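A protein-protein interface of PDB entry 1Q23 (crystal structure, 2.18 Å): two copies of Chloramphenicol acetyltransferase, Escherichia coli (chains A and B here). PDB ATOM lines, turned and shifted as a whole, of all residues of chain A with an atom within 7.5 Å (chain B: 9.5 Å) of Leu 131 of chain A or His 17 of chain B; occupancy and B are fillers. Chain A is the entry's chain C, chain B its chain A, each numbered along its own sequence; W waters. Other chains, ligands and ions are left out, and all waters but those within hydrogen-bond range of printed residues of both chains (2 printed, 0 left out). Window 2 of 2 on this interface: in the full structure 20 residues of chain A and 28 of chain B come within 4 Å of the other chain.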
ATOM      1  N   HIS A  96      16.802 -30.597  -9.144  1.00  0.00           N
ATOM      2  CA  HIS A  96      17.575 -31.437 -10.135  1.00  0.00           C
ATOM      3  C   HIS A  96      19.041 -31.365  -9.763  1.00  0.00           C
ATOM      4  O   HIS A  96      19.666 -30.389 -10.041  1.00  0.00           O
ATOM      5  CB  HIS A  96      17.400 -30.966 -11.543  1.00  0.00           C
ATOM      6  CG  HIS A  96      15.976 -30.783 -11.933  1.00  0.00           C
ATOM      7  ND1 HIS A  96      15.102 -31.840 -12.057  1.00  0.00           N
ATOM      8  CD2 HIS A  96      15.260 -29.672 -12.211  1.00  0.00           C
ATOM      9  CE1 HIS A  96      13.912 -31.385 -12.411  1.00  0.00           C
ATOM     10  NE2 HIS A  96      13.976 -30.074 -12.484  1.00  0.00           N
ATOM     11  N   GLU A  97      19.549 -32.404  -9.090  1.00  0.00           N
ATOM     12  CA  GLU A  97      20.878 -32.368  -8.458  1.00  0.00           C
ATOM     13  C   GLU A  97      21.943 -32.142  -9.482  1.00  0.00           C
ATOM     14  O   GLU A  97      22.965 -31.535  -9.137  1.00  0.00           O
ATOM     15  CB  GLU A  97      21.219 -33.658  -7.711  1.00  0.00           C
ATOM     16  CG  GLU A  97      20.688 -33.688  -6.252  1.00  0.00           C
ATOM     17  CD  GLU A  97      20.968 -35.053  -5.580  1.00  0.00           C
ATOM     18  OE1 GLU A  97      21.870 -35.767  -6.082  1.00  0.00           O
ATOM     19  OE2 GLU A  97      20.308 -35.441  -4.571  1.00  0.00           O
ATOM     20  N   GLN A  98      21.705 -32.630 -10.709  1.00  0.00           N
ATOM     21  CA  GLN A  98      22.679 -32.570 -11.772  1.00  0.00           C
ATOM     22  C   GLN A  98      22.842 -31.203 -12.473  1.00  0.00           C
ATOM     23  O   GLN A  98      23.928 -30.887 -12.938  1.00  0.00           O
ATOM     24  CB  GLN A  98      22.421 -33.644 -12.891  1.00  0.00           C
ATOM     25  CG  GLN A  98      22.426 -35.212 -12.486  1.00  0.00           C
ATOM     26  CD  GLN A  98      23.650 -35.735 -11.654  1.00  0.00           C
ATOM     27  OE1 GLN A  98      23.457 -36.599 -10.741  1.00  0.00           O
ATOM     28  NE2 GLN A  98      24.898 -35.238 -11.971  1.00  0.00           N
ATOM     29  N   THR A  99      21.779 -30.411 -12.593  1.00  0.00           N
ATOM     30  CA  THR A  99      21.931 -29.095 -13.150  1.00  0.00           C
ATOM     31  C   THR A  99      21.813 -28.043 -12.047  1.00  0.00           C
ATOM     32  O   THR A  99      22.028 -26.844 -12.329  1.00  0.00           O
ATOM     33  CB  THR A  99      20.790 -28.858 -14.130  1.00  0.00           C
ATOM     34  OG1 THR A  99      19.633 -29.140 -13.372  1.00  0.00           O
ATOM     35  CG2 THR A  99      20.793 -29.905 -15.281  1.00  0.00           C
ATOM     36  N   GLU A 100      21.467 -28.457 -10.802  1.00  0.00           N
ATOM     37  CA  GLU A 100      21.352 -27.490  -9.709  1.00  0.00           C
ATOM     38  C   GLU A 100      20.303 -26.439 -10.029  1.00  0.00           C
ATOM     39  O   GLU A 100      20.438 -25.260  -9.715  1.00  0.00           O
ATOM     40  CB  GLU A 100      22.762 -26.811  -9.491  1.00  0.00           C
ATOM     41  CG  GLU A 100      23.689 -27.816  -8.798  1.00  0.00           C
ATOM     42  CD  GLU A 100      25.122 -27.330  -8.723  1.00  0.00           C
ATOM     43  OE1 GLU A 100      25.409 -26.218  -9.270  1.00  0.00           O
ATOM     44  OE2 GLU A 100      25.903 -28.090  -8.067  1.00  0.00           O
ATOM     45  N   THR A 101      19.248 -26.864 -10.668  1.00  0.00           N
ATOM     46  CA  THR A 101      18.165 -25.993 -10.849  1.00  0.00           C
ATOM     47  C   THR A 101      16.927 -26.689 -10.331  1.00  0.00           C
ATOM     48  O   THR A 101      17.014 -27.884  -9.908  1.00  0.00           O
ATOM     49  CB  THR A 101      17.985 -25.706 -12.320  1.00  0.00           C
ATOM     50  OG1 THR A 101      17.759 -26.955 -12.962  1.00  0.00           O
ATOM     51  CG2 THR A 101      19.237 -25.159 -12.925  1.00  0.00           C
ATOM     52  N   PHE A 102      15.780 -25.991 -10.376  1.00  0.00           N
ATOM     53  CA  PHE A 102      14.595 -26.592  -9.799  1.00  0.00           C
ATOM     54  C   PHE A 102      13.421 -26.431 -10.742  1.00  0.00           C
ATOM     55  O   PHE A 102      13.495 -25.630 -11.694  1.00  0.00           O
ATOM     56  CB  PHE A 102      14.274 -25.962  -8.391  1.00  0.00           C
ATOM     57  CG  PHE A 102      13.603 -24.559  -8.491  1.00  0.00           C
ATOM     58  CD1 PHE A 102      12.255 -24.432  -8.316  1.00  0.00           C
ATOM     59  CD2 PHE A 102      14.345 -23.432  -8.736  1.00  0.00           C
ATOM     60  CE1 PHE A 102      11.600 -23.220  -8.384  1.00  0.00           C
ATOM     61  CE2 PHE A 102      13.741 -22.169  -8.801  1.00  0.00           C
ATOM     62  CZ  PHE A 102      12.335 -22.056  -8.650  1.00  0.00           C
ATOM     63  N   SER A 103      12.339 -27.168 -10.457  1.00  0.00           N
ATOM     64  CA  SER A 103      11.084 -26.982 -11.200  1.00  0.00           C
ATOM     65  C   SER A 103       9.966 -26.929 -10.167  1.00  0.00           C
ATOM     66  O   SER A 103      10.097 -27.333  -8.976  1.00  0.00           O
ATOM     67  CB  SER A 103      10.834 -28.132 -12.147  1.00  0.00           C
ATOM     68  OG  SER A 103      11.979 -28.391 -13.015  1.00  0.00           O
ATOM     69  N   TYR A 127       7.533 -36.368 -14.666  1.00  0.00           N
ATOM     70  CA  TYR A 127       8.105 -35.073 -14.905  1.00  0.00           C
ATOM     71  C   TYR A 127       9.260 -34.710 -14.066  1.00  0.00           C
ATOM     72  O   TYR A 127       9.749 -33.589 -14.207  1.00  0.00           O
ATOM     73  CB  TYR A 127       7.098 -34.016 -14.602  1.00  0.00           C
ATOM     74  CG  TYR A 127       5.919 -34.100 -15.422  1.00  0.00           C
ATOM     75  CD1 TYR A 127       5.938 -33.544 -16.680  1.00  0.00           C
ATOM     76  CD2 TYR A 127       4.735 -34.754 -14.938  1.00  0.00           C
ATOM     77  CE1 TYR A 127       4.827 -33.599 -17.494  1.00  0.00           C
ATOM     78  CE2 TYR A 127       3.617 -34.798 -15.714  1.00  0.00           C
ATOM     79  CZ  TYR A 127       3.681 -34.222 -16.991  1.00  0.00           C
ATOM     80  OH  TYR A 127       2.588 -34.279 -17.775  1.00  0.00           O
ATOM     81  N   GLY A 128       9.742 -35.585 -13.201  1.00  0.00           N
ATOM     82  CA  GLY A 128      10.818 -35.128 -12.346  1.00  0.00           C
ATOM     83  C   GLY A 128      12.198 -34.777 -12.933  1.00  0.00           C
ATOM     84  O   GLY A 128      13.036 -34.150 -12.200  1.00  0.00           O
ATOM     85  N   GLU A 129      12.458 -35.145 -14.187  1.00  0.00           N
ATOM     86  CA  GLU A 129      13.741 -34.934 -14.898  1.00  0.00           C
ATOM     87  C   GLU A 129      13.600 -33.812 -15.921  1.00  0.00           C
ATOM     88  O   GLU A 129      14.538 -33.390 -16.561  1.00  0.00           O
ATOM     89  CB  GLU A 129      14.117 -36.203 -15.727  1.00  0.00           C
ATOM     90  CG  GLU A 129      14.469 -37.476 -14.844  1.00  0.00           C
ATOM     91  CD  GLU A 129      15.565 -37.126 -13.845  1.00  0.00           C
ATOM     92  OE1 GLU A 129      16.540 -36.500 -14.274  1.00  0.00           O
ATOM     93  OE2 GLU A 129      15.457 -37.411 -12.645  1.00  0.00           O
ATOM     94  N   ASN A 130      12.391 -33.361 -16.069  1.00  0.00           N
ATOM     95  CA  ASN A 130      12.144 -32.314 -16.960  1.00  0.00           C
ATOM     96  C   ASN A 130      12.580 -30.989 -16.291  1.00  0.00           C
ATOM     97  O   ASN A 130      12.136 -30.663 -15.164  1.00  0.00           O
ATOM     98  CB  ASN A 130      10.678 -32.422 -17.277  1.00  0.00           C
ATOM     99  CG  ASN A 130      10.236 -31.451 -18.213  1.00  0.00           C
ATOM    100  OD1 ASN A 130      10.787 -30.356 -18.295  1.00  0.00           O
ATOM    101  ND2 ASN A 130       9.195 -31.796 -18.947  1.00  0.00           N
ATOM    102  N   LEU A 131      13.448 -30.244 -16.995  1.00  0.00           N
ATOM    103  CA  LEU A 131      14.052 -29.043 -16.494  1.00  0.00           C
ATOM    104  C   LEU A 131      13.312 -27.779 -16.727  1.00  0.00           C
ATOM    105  O   LEU A 131      13.877 -26.716 -16.417  1.00  0.00           O
ATOM    106  CB  LEU A 131      15.515 -28.839 -16.957  1.00  0.00           C
ATOM    107  CG  LEU A 131      16.482 -30.044 -17.040  1.00  0.00           C
ATOM    108  CD1 LEU A 131      17.786 -29.597 -17.872  1.00  0.00           C
ATOM    109  CD2 LEU A 131      16.901 -30.520 -15.668  1.00  0.00           C
ATOM    110  N   ALA A 132      12.083 -27.862 -17.270  1.00  0.00           N
ATOM    111  CA  ALA A 132      11.252 -26.685 -17.427  1.00  0.00           C
ATOM    112  C   ALA A 132      11.031 -26.127 -16.002  1.00  0.00           C
ATOM    113  O   ALA A 132      11.057 -26.867 -14.960  1.00  0.00           O
ATOM    114  CB  ALA A 132       9.931 -27.060 -18.035  1.00  0.00           C
ATOM    115  N   TYR A 133      10.859 -24.845 -15.953  1.00  0.00           N
ATOM    116  CA  TYR A 133      10.507 -24.202 -14.795  1.00  0.00           C
ATOM    117  C   TYR A 133       9.124 -24.805 -14.393  1.00  0.00           C
ATOM    118  O   TYR A 133       8.943 -25.374 -13.203  1.00  0.00           O
ATOM    119  CB  TYR A 133      10.581 -22.682 -15.007  1.00  0.00           C
ATOM    120  CG  TYR A 133      10.123 -21.852 -13.829  1.00  0.00           C
ATOM    121  CD1 TYR A 133      10.247 -22.312 -12.489  1.00  0.00           C
ATOM    122  CD2 TYR A 133       9.572 -20.630 -14.026  1.00  0.00           C
ATOM    123  CE1 TYR A 133       9.769 -21.506 -11.367  1.00  0.00           C
ATOM    124  CE2 TYR A 133       9.116 -19.836 -12.939  1.00  0.00           C
ATOM    125  CZ  TYR A 133       9.232 -20.312 -11.626  1.00  0.00           C
ATOM    126  OH  TYR A 133       8.734 -19.508 -10.676  1.00  0.00           O
ATOM    127  N   PHE A 134       8.168 -24.758 -15.332  1.00  0.00           N
ATOM    128  CA  PHE A 134       6.874 -25.456 -15.082  1.00  0.00           C
ATOM    129  C   PHE A 134       6.570 -26.620 -16.099  1.00  0.00           C
ATOM    130  O   PHE A 134       5.844 -26.416 -17.081  1.00  0.00           O
ATOM    131  CB  PHE A 134       5.730 -24.458 -15.112  1.00  0.00           C
ATOM    132  CG  PHE A 134       5.599 -23.594 -13.840  1.00  0.00           C
ATOM    133  CD1 PHE A 134       6.321 -22.375 -13.715  1.00  0.00           C
ATOM    134  CD2 PHE A 134       4.743 -23.982 -12.801  1.00  0.00           C
ATOM    135  CE1 PHE A 134       6.173 -21.583 -12.547  1.00  0.00           C
ATOM    136  CE2 PHE A 134       4.585 -23.215 -11.637  1.00  0.00           C
ATOM    137  CZ  PHE A 134       5.310 -22.018 -11.511  1.00  0.00           C
ATOM    138  N   PRO A 135       7.090 -27.802 -15.825  1.00  0.00           N
ATOM    139  CA  PRO A 135       6.905 -28.996 -16.675  1.00  0.00           C
ATOM    140  C   PRO A 135       5.412 -29.305 -17.035  1.00  0.00           C
ATOM    141  O   PRO A 135       5.214 -29.817 -18.139  1.00  0.00           O
ATOM    142  CB  PRO A 135       7.489 -30.172 -15.823  1.00  0.00           C
ATOM    143  CG  PRO A 135       8.411 -29.566 -14.946  1.00  0.00           C
ATOM    144  CD  PRO A 135       7.883 -28.115 -14.615  1.00  0.00           C
ATOM    145  N   VAL B  11      26.888 -13.930 -19.212  1.00  0.00           N
ATOM    146  CA  VAL B  11      26.113 -15.204 -19.171  1.00  0.00           C
ATOM    147  C   VAL B  11      25.396 -15.386 -20.527  1.00  0.00           C
ATOM    148  O   VAL B  11      24.734 -14.486 -21.029  1.00  0.00           O
ATOM    149  CB  VAL B  11      25.068 -15.152 -18.142  1.00  0.00           C
ATOM    150  CG1 VAL B  11      24.313 -16.375 -18.142  1.00  0.00           C
ATOM    151  CG2 VAL B  11      25.728 -14.981 -16.681  1.00  0.00           C
ATOM    152  N   ASP B  12      25.537 -16.545 -21.116  1.00  0.00           N
ATOM    153  CA  ASP B  12      24.697 -16.830 -22.244  1.00  0.00           C
ATOM    154  C   ASP B  12      23.300 -17.403 -21.884  1.00  0.00           C
ATOM    155  O   ASP B  12      23.119 -18.612 -21.656  1.00  0.00           O
ATOM    156  CB  ASP B  12      25.393 -17.783 -23.207  1.00  0.00           C
ATOM    157  CG  ASP B  12      24.527 -17.987 -24.492  1.00  0.00           C
ATOM    158  OD1 ASP B  12      25.007 -18.657 -25.359  1.00  0.00           O
ATOM    159  OD2 ASP B  12      23.343 -17.512 -24.671  1.00  0.00           O
ATOM    160  N   ILE B  13      22.316 -16.549 -21.873  1.00  0.00           N
ATOM    161  CA  ILE B  13      21.011 -16.945 -21.468  1.00  0.00           C
ATOM    162  C   ILE B  13      20.391 -17.998 -22.288  1.00  0.00           C
ATOM    163  O   ILE B  13      19.735 -18.813 -21.741  1.00  0.00           O
ATOM    164  CB  ILE B  13      20.137 -15.764 -21.331  1.00  0.00           C
ATOM    165  CG1 ILE B  13      20.812 -14.759 -20.354  1.00  0.00           C
ATOM    166  CG2 ILE B  13      18.836 -16.166 -20.819  1.00  0.00           C
ATOM    167  CD1 ILE B  13      19.904 -13.693 -19.775  1.00  0.00           C
ATOM    168  N   SER B  14      20.586 -18.037 -23.606  1.00  0.00           N
ATOM    169  CA  SER B  14      19.827 -19.042 -24.415  1.00  0.00           C
ATOM    170  C   SER B  14      20.368 -20.457 -24.123  1.00  0.00           C
ATOM    171  O   SER B  14      19.733 -21.494 -24.388  1.00  0.00           O
ATOM    172  CB  SER B  14      20.009 -18.784 -25.903  1.00  0.00           C
ATOM    173  OG  SER B  14      21.397 -18.534 -26.162  1.00  0.00           O
ATOM    174  N   GLN B  15      21.561 -20.510 -23.567  1.00  0.00           N
ATOM    175  CA  GLN B  15      22.124 -21.828 -23.254  1.00  0.00           C
ATOM    176  C   GLN B  15      22.077 -22.183 -21.800  1.00  0.00           C
ATOM    177  O   GLN B  15      22.636 -23.189 -21.430  1.00  0.00           O
ATOM    178  CB  GLN B  15      23.564 -21.891 -23.710  1.00  0.00           C
ATOM    179  CG  GLN B  15      23.685 -21.764 -25.218  1.00  0.00           C
ATOM    180  CD  GLN B  15      23.037 -22.897 -25.883  1.00  0.00           C
ATOM    181  OE1 GLN B  15      23.455 -24.057 -25.667  1.00  0.00           O
ATOM    182  NE2 GLN B  15      21.980 -22.613 -26.670  1.00  0.00           N
ATOM    183  N   TRP B  16      21.443 -21.371 -20.973  1.00  0.00           N
ATOM    184  CA  TRP B  16      21.540 -21.539 -19.530  1.00  0.00           C
ATOM    185  C   TRP B  16      20.410 -22.383 -18.956  1.00  0.00           C
ATOM    186  O   TRP B  16      19.204 -22.220 -19.357  1.00  0.00           O
ATOM    187  CB  TRP B  16      21.499 -20.130 -18.989  1.00  0.00           C
ATOM    188  CG  TRP B  16      21.793 -19.930 -17.612  1.00  0.00           C
ATOM    189  CD1 TRP B  16      22.520 -20.764 -16.770  1.00  0.00           C
ATOM    190  CD2 TRP B  16      21.389 -18.826 -16.814  1.00  0.00           C
ATOM    191  NE1 TRP B  16      22.590 -20.221 -15.512  1.00  0.00           N
ATOM    192  CE2 TRP B  16      21.909 -19.042 -15.493  1.00  0.00           C
ATOM    193  CE3 TRP B  16      20.669 -17.670 -17.064  1.00  0.00           C
ATOM    194  CZ2 TRP B  16      21.691 -18.120 -14.407  1.00  0.00           C
ATOM    195  CZ3 TRP B  16      20.429 -16.761 -15.998  1.00  0.00           C
ATOM    196  CH2 TRP B  16      20.938 -16.998 -14.672  1.00  0.00           C
ATOM    197  N   HIS B  17      20.704 -23.263 -17.990  1.00  0.00           N
ATOM    198  CA  HIS B  17      19.583 -24.102 -17.551  1.00  0.00           C
ATOM    199  C   HIS B  17      18.652 -23.243 -16.717  1.00  0.00           C
ATOM    200  O   HIS B  17      17.505 -23.698 -16.438  1.00  0.00           O
ATOM    201  CB  HIS B  17      19.987 -25.317 -16.735  1.00  0.00           C
ATOM    202  CG  HIS B  17      20.676 -26.362 -17.544  1.00  0.00           C
ATOM    203  ND1 HIS B  17      20.147 -26.832 -18.725  1.00  0.00           N
ATOM    204  CD2 HIS B  17      21.842 -27.039 -17.340  1.00  0.00           C
ATOM    205  CE1 HIS B  17      20.969 -27.742 -19.237  1.00  0.00           C
ATOM    206  NE2 HIS B  17      21.999 -27.894 -18.411  1.00  0.00           N
ATOM    207  N   ARG B  18      19.083 -22.009 -16.381  1.00  0.00           N
ATOM    208  CA  ARG B  18      18.129 -21.139 -15.640  1.00  0.00           C
ATOM    209  C   ARG B  18      17.471 -20.118 -16.543  1.00  0.00           C
ATOM    210  O   ARG B  18      16.795 -19.267 -16.022  1.00  0.00           O
ATOM    211  CB  ARG B  18      18.693 -20.419 -14.409  1.00  0.00           C
ATOM    212  CG  ARG B  18      19.200 -21.415 -13.351  1.00  0.00           C
ATOM    213  CD  ARG B  18      19.625 -20.873 -11.913  1.00  0.00           C
ATOM    214  NE  ARG B  18      18.553 -20.129 -11.211  1.00  0.00           N
ATOM    215  CZ  ARG B  18      18.378 -18.785 -11.304  1.00  0.00           C
ATOM    216  NH1 ARG B  18      19.149 -18.005 -12.069  1.00  0.00           N
ATOM    217  NH2 ARG B  18      17.377 -18.232 -10.640  1.00  0.00           N
ATOM    218  N   LYS B  19      17.621 -20.247 -17.867  1.00  0.00           N
ATOM    219  CA  LYS B  19      16.970 -19.275 -18.815  1.00  0.00           C
ATOM    220  C   LYS B  19      15.532 -18.951 -18.377  1.00  0.00           C
ATOM    221  O   LYS B  19      15.190 -17.777 -18.108  1.00  0.00           O
ATOM    222  CB  LYS B  19      17.037 -19.795 -20.270  1.00  0.00           C
ATOM    223  CG  LYS B  19      16.368 -18.861 -21.420  1.00  0.00           C
ATOM    224  CD  LYS B  19      16.249 -19.725 -22.805  1.00  0.00           C
ATOM    225  CE  LYS B  19      15.807 -18.798 -23.948  1.00  0.00           C
ATOM    226  NZ  LYS B  19      14.584 -18.126 -23.415  1.00  0.00           N
ATOM    227  N   GLU B  20      14.692 -19.970 -18.259  1.00  0.00           N
ATOM    228  CA  GLU B  20      13.261 -19.761 -17.921  1.00  0.00           C
ATOM    229  C   GLU B  20      13.048 -19.072 -16.599  1.00  0.00           C
ATOM    230  O   GLU B  20      12.213 -18.142 -16.507  1.00  0.00           O
ATOM    231  CB  GLU B  20      12.507 -21.059 -17.886  1.00  0.00           C
ATOM    232  CG  GLU B  20      12.047 -21.532 -19.286  1.00  0.00           C
ATOM    233  CD  GLU B  20      11.494 -22.973 -19.319  1.00  0.00           C
ATOM    234  OE1 GLU B  20      11.457 -23.555 -20.439  1.00  0.00           O
ATOM    235  OE2 GLU B  20      11.108 -23.538 -18.266  1.00  0.00           O
ATOM    236  N   HIS B  21      13.813 -19.514 -15.593  1.00  0.00           N
ATOM    237  CA  HIS B  21      13.677 -18.957 -14.247  1.00  0.00           C
ATOM    238  C   HIS B  21      14.087 -17.523 -14.312  1.00  0.00           C
ATOM    239  O   HIS B  21      13.359 -16.683 -13.852  1.00  0.00           O
ATOM    240  CB  HIS B  21      14.537 -19.737 -13.218  1.00  0.00           C
ATOM    241  CG  HIS B  21      14.365 -21.196 -13.307  1.00  0.00           C
ATOM    242  ND1 HIS B  21      14.865 -21.934 -14.375  1.00  0.00           N
ATOM    243  CD2 HIS B  21      13.785 -22.093 -12.457  1.00  0.00           C
ATOM    244  CE1 HIS B  21      14.573 -23.217 -14.184  1.00  0.00           C
ATOM    245  NE2 HIS B  21      13.935 -23.345 -13.028  1.00  0.00           N
ATOM    246  N   PHE B  22      15.246 -17.222 -14.923  1.00  0.00           N
ATOM    247  CA  PHE B  22      15.723 -15.843 -15.000  1.00  0.00           C
ATOM    248  C   PHE B  22      14.633 -14.960 -15.679  1.00  0.00           C
ATOM    249  O   PHE B  22      14.341 -13.808 -15.212  1.00  0.00           O
ATOM    250  CB  PHE B  22      17.076 -15.743 -15.754  1.00  0.00           C
ATOM    251  CG  PHE B  22      17.595 -14.324 -15.922  1.00  0.00           C
ATOM    252  CD1 PHE B  22      17.485 -13.650 -17.164  1.00  0.00           C
ATOM    253  CD2 PHE B  22      18.250 -13.685 -14.880  1.00  0.00           C
ATOM    254  CE1 PHE B  22      17.966 -12.260 -17.373  1.00  0.00           C
ATOM    255  CE2 PHE B  22      18.747 -12.382 -15.023  1.00  0.00           C
ATOM    256  CZ  PHE B  22      18.583 -11.623 -16.374  1.00  0.00           C
ATOM    257  N   GLU B  23      14.044 -15.495 -16.731  1.00  0.00           N
ATOM    258  CA  GLU B  23      13.137 -14.683 -17.525  1.00  0.00           C
ATOM    259  C   GLU B  23      11.902 -14.375 -16.740  1.00  0.00           C
ATOM    260  O   GLU B  23      11.400 -13.245 -16.755  1.00  0.00           O
ATOM    261  CB  GLU B  23      12.734 -15.495 -18.725  1.00  0.00           C
ATOM    262  CG  GLU B  23      13.792 -15.215 -19.803  1.00  0.00           C
ATOM    263  CD  GLU B  23      13.717 -16.144 -21.082  1.00  0.00           C
ATOM    264  OE1 GLU B  23      12.838 -17.046 -21.205  1.00  0.00           O
ATOM    265  OE2 GLU B  23      14.567 -15.970 -21.987  1.00  0.00           O
ATOM    266  N   ALA B 194      16.152 -13.788  -9.334  1.00  0.00           N
ATOM    267  CA  ALA B 194      16.571 -13.925 -10.750  1.00  0.00           C
ATOM    268  C   ALA B 194      17.983 -14.534 -10.822  1.00  0.00           C
ATOM    269  O   ALA B 194      18.335 -15.190 -11.747  1.00  0.00           O
ATOM    270  CB  ALA B 194      16.496 -12.556 -11.496  1.00  0.00           C
ATOM    271  N   ASP B 197      18.689 -19.168  -6.439  1.00  0.00           N
ATOM    272  CA  ASP B 197      17.582 -20.030  -5.935  1.00  0.00           C
ATOM    273  C   ASP B 197      18.011 -20.473  -4.493  1.00  0.00           C
ATOM    274  O   ASP B 197      19.071 -20.135  -4.104  1.00  0.00           O
ATOM    275  CB  ASP B 197      17.463 -21.291  -6.817  1.00  0.00           C
ATOM    276  CG  ASP B 197      17.121 -20.933  -8.262  1.00  0.00           C
ATOM    277  OD1 ASP B 197      17.553 -21.547  -9.264  1.00  0.00           O
ATOM    278  OD2 ASP B 197      16.455 -19.937  -8.439  1.00  0.00           O
ATOM    279  N   HIS B 200      21.361 -22.090  -3.974  1.00  0.00           N
ATOM    280  CA  HIS B 200      22.625 -21.210  -3.919  1.00  0.00           C
ATOM    281  C   HIS B 200      22.834 -20.628  -2.560  1.00  0.00           C
ATOM    282  O   HIS B 200      23.992 -20.690  -2.083  1.00  0.00           O
ATOM    283  CB  HIS B 200      22.623 -20.145  -5.031  1.00  0.00           C
ATOM    284  CG  HIS B 200      22.429 -20.786  -6.365  1.00  0.00           C
ATOM    285  ND1 HIS B 200      21.191 -20.910  -6.978  1.00  0.00           N
ATOM    286  CD2 HIS B 200      23.313 -21.418  -7.163  1.00  0.00           C
ATOM    287  CE1 HIS B 200      21.354 -21.518  -8.123  1.00  0.00           C
ATOM    288  NE2 HIS B 200      22.626 -21.840  -8.256  1.00  0.00           N
HETATM  289  O   HOH W   1      16.482 -23.013 -11.136  1.00  0.00           O
HETATM  290  O   HOH W   2      18.520 -24.030  -8.083  1.00  0.00           O
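OE2 of Glu 20 of chain B sits at hydrogen-bond distance from N of Tyr 133 of chain A (2.7 Å). A ring nitrogen (NE2) of His 21 of chain B lies within hydrogen-bond range of the backbone carbonyl oxygen (O) of Phe 102 of chain A, 2.7 Å away.
The guanidinium group (NH1) of Arg 18 of chain B is in hydrogen-bond range of the backbone carbonyl oxygen (O) of Ala 194 of chain B (2.9 Å). OD1 of Asp 197 of chain B is in salt-bridge range of NE of Arg 18 of chain B (2.6 Å). N of His 96 of chain A sits at hydrogen-bond distance from O of Thr 101 of chain A, at 2.8 Å. The side-chain hydroxyl of Thr 101 of chain A lies within hydrogen-bond range of the side-chain hydroxyl of Thr 99 of chain A (2.9 Å). The backbone carbonyl oxygen of Ala 132 of chain A lies within hydrogen-bond range of the side-chain hydroxyl of Ser 103 of chain A (2.6 Å). OD1 of Asn 130 of chain A is in hydrogen-bond range of N of Ala 132 of chain A (3.0 Å).
His 17 of chain B touches Thr 99 of chain A (CD2 to CG2, 3.7 Å). His 17 of chain B touches Thr 101 of chain A. Thr 101 of chain A touches Arg 18 of chain B (CG2 to CG, 3.8 Å). Asp 197 of chain B touches Phe 102 of chain A. ND1 of His 17 of chain B touches CD1 of Leu 131 of chain A, at 3.7 Å. Ala 132 of chain A touches Glu 20 of chain B (CA to OE2, 3.3 Å). His 21 of chain B touches Tyr 133 of chain A (CD2 to CD1, 3.5 Å).
Printed residues of chain B within 4 Å of Phe 102 of chain A: His 21 and Asp 197. No residue of chain B comes within 4 Å of Asn 130 of chain A. Of chain B, only His 17 (3.7 Å) comes within 4 Å of Leu 131 of chain A. Ala 132 of chain A touches just one residue of chain B: Glu 20. Of the printed residues of chain B, Tyr 133 of chain A touches Glu 20 (2.7 Å) and His 21 (3.5 Å). Ser 14 of chain B touches none of the printed residues of chain A. Of the printed residues of chain A, His 17 of chain B touches Thr 99 (3.7 Å), Thr 101 (3.9 Å) and Leu 131 (3.7 Å). Of the printed residues of chain A, Glu 20 of chain B touches Ala 132 (3.3 Å) and Tyr 133 (2.7 Å). Glu 23 of chain B touches none of the printed residues of chain A.
Of the 16 printed residues of chain B, 5 touch a printed residue of chain A. Hydrophobic or aromatic side chains of chain B that line the printed part of chain A: His 17 and His 21. Hydrophobic or aromatic side chains of chain A within 4 Å of the printed part of chain B: Phe 102, Leu 131, Ala 132 and Tyr 133. Among the printed residues, no Asp or Glu carboxylate lies within 4 Å of a Lys or Arg side-chain nitrogen of the other chain.
No position is printed for both chains.
Water W1 lies within hydrogen-bond range of OD1 of Asp 197 of chain B, N of Phe 102 of chain A and NE2 of His 21 of chain B. Water W2 bridges O of Glu 100 of chain A (2.8 Å) and OD1 of Asp 197 of chain B (2.9 Å).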
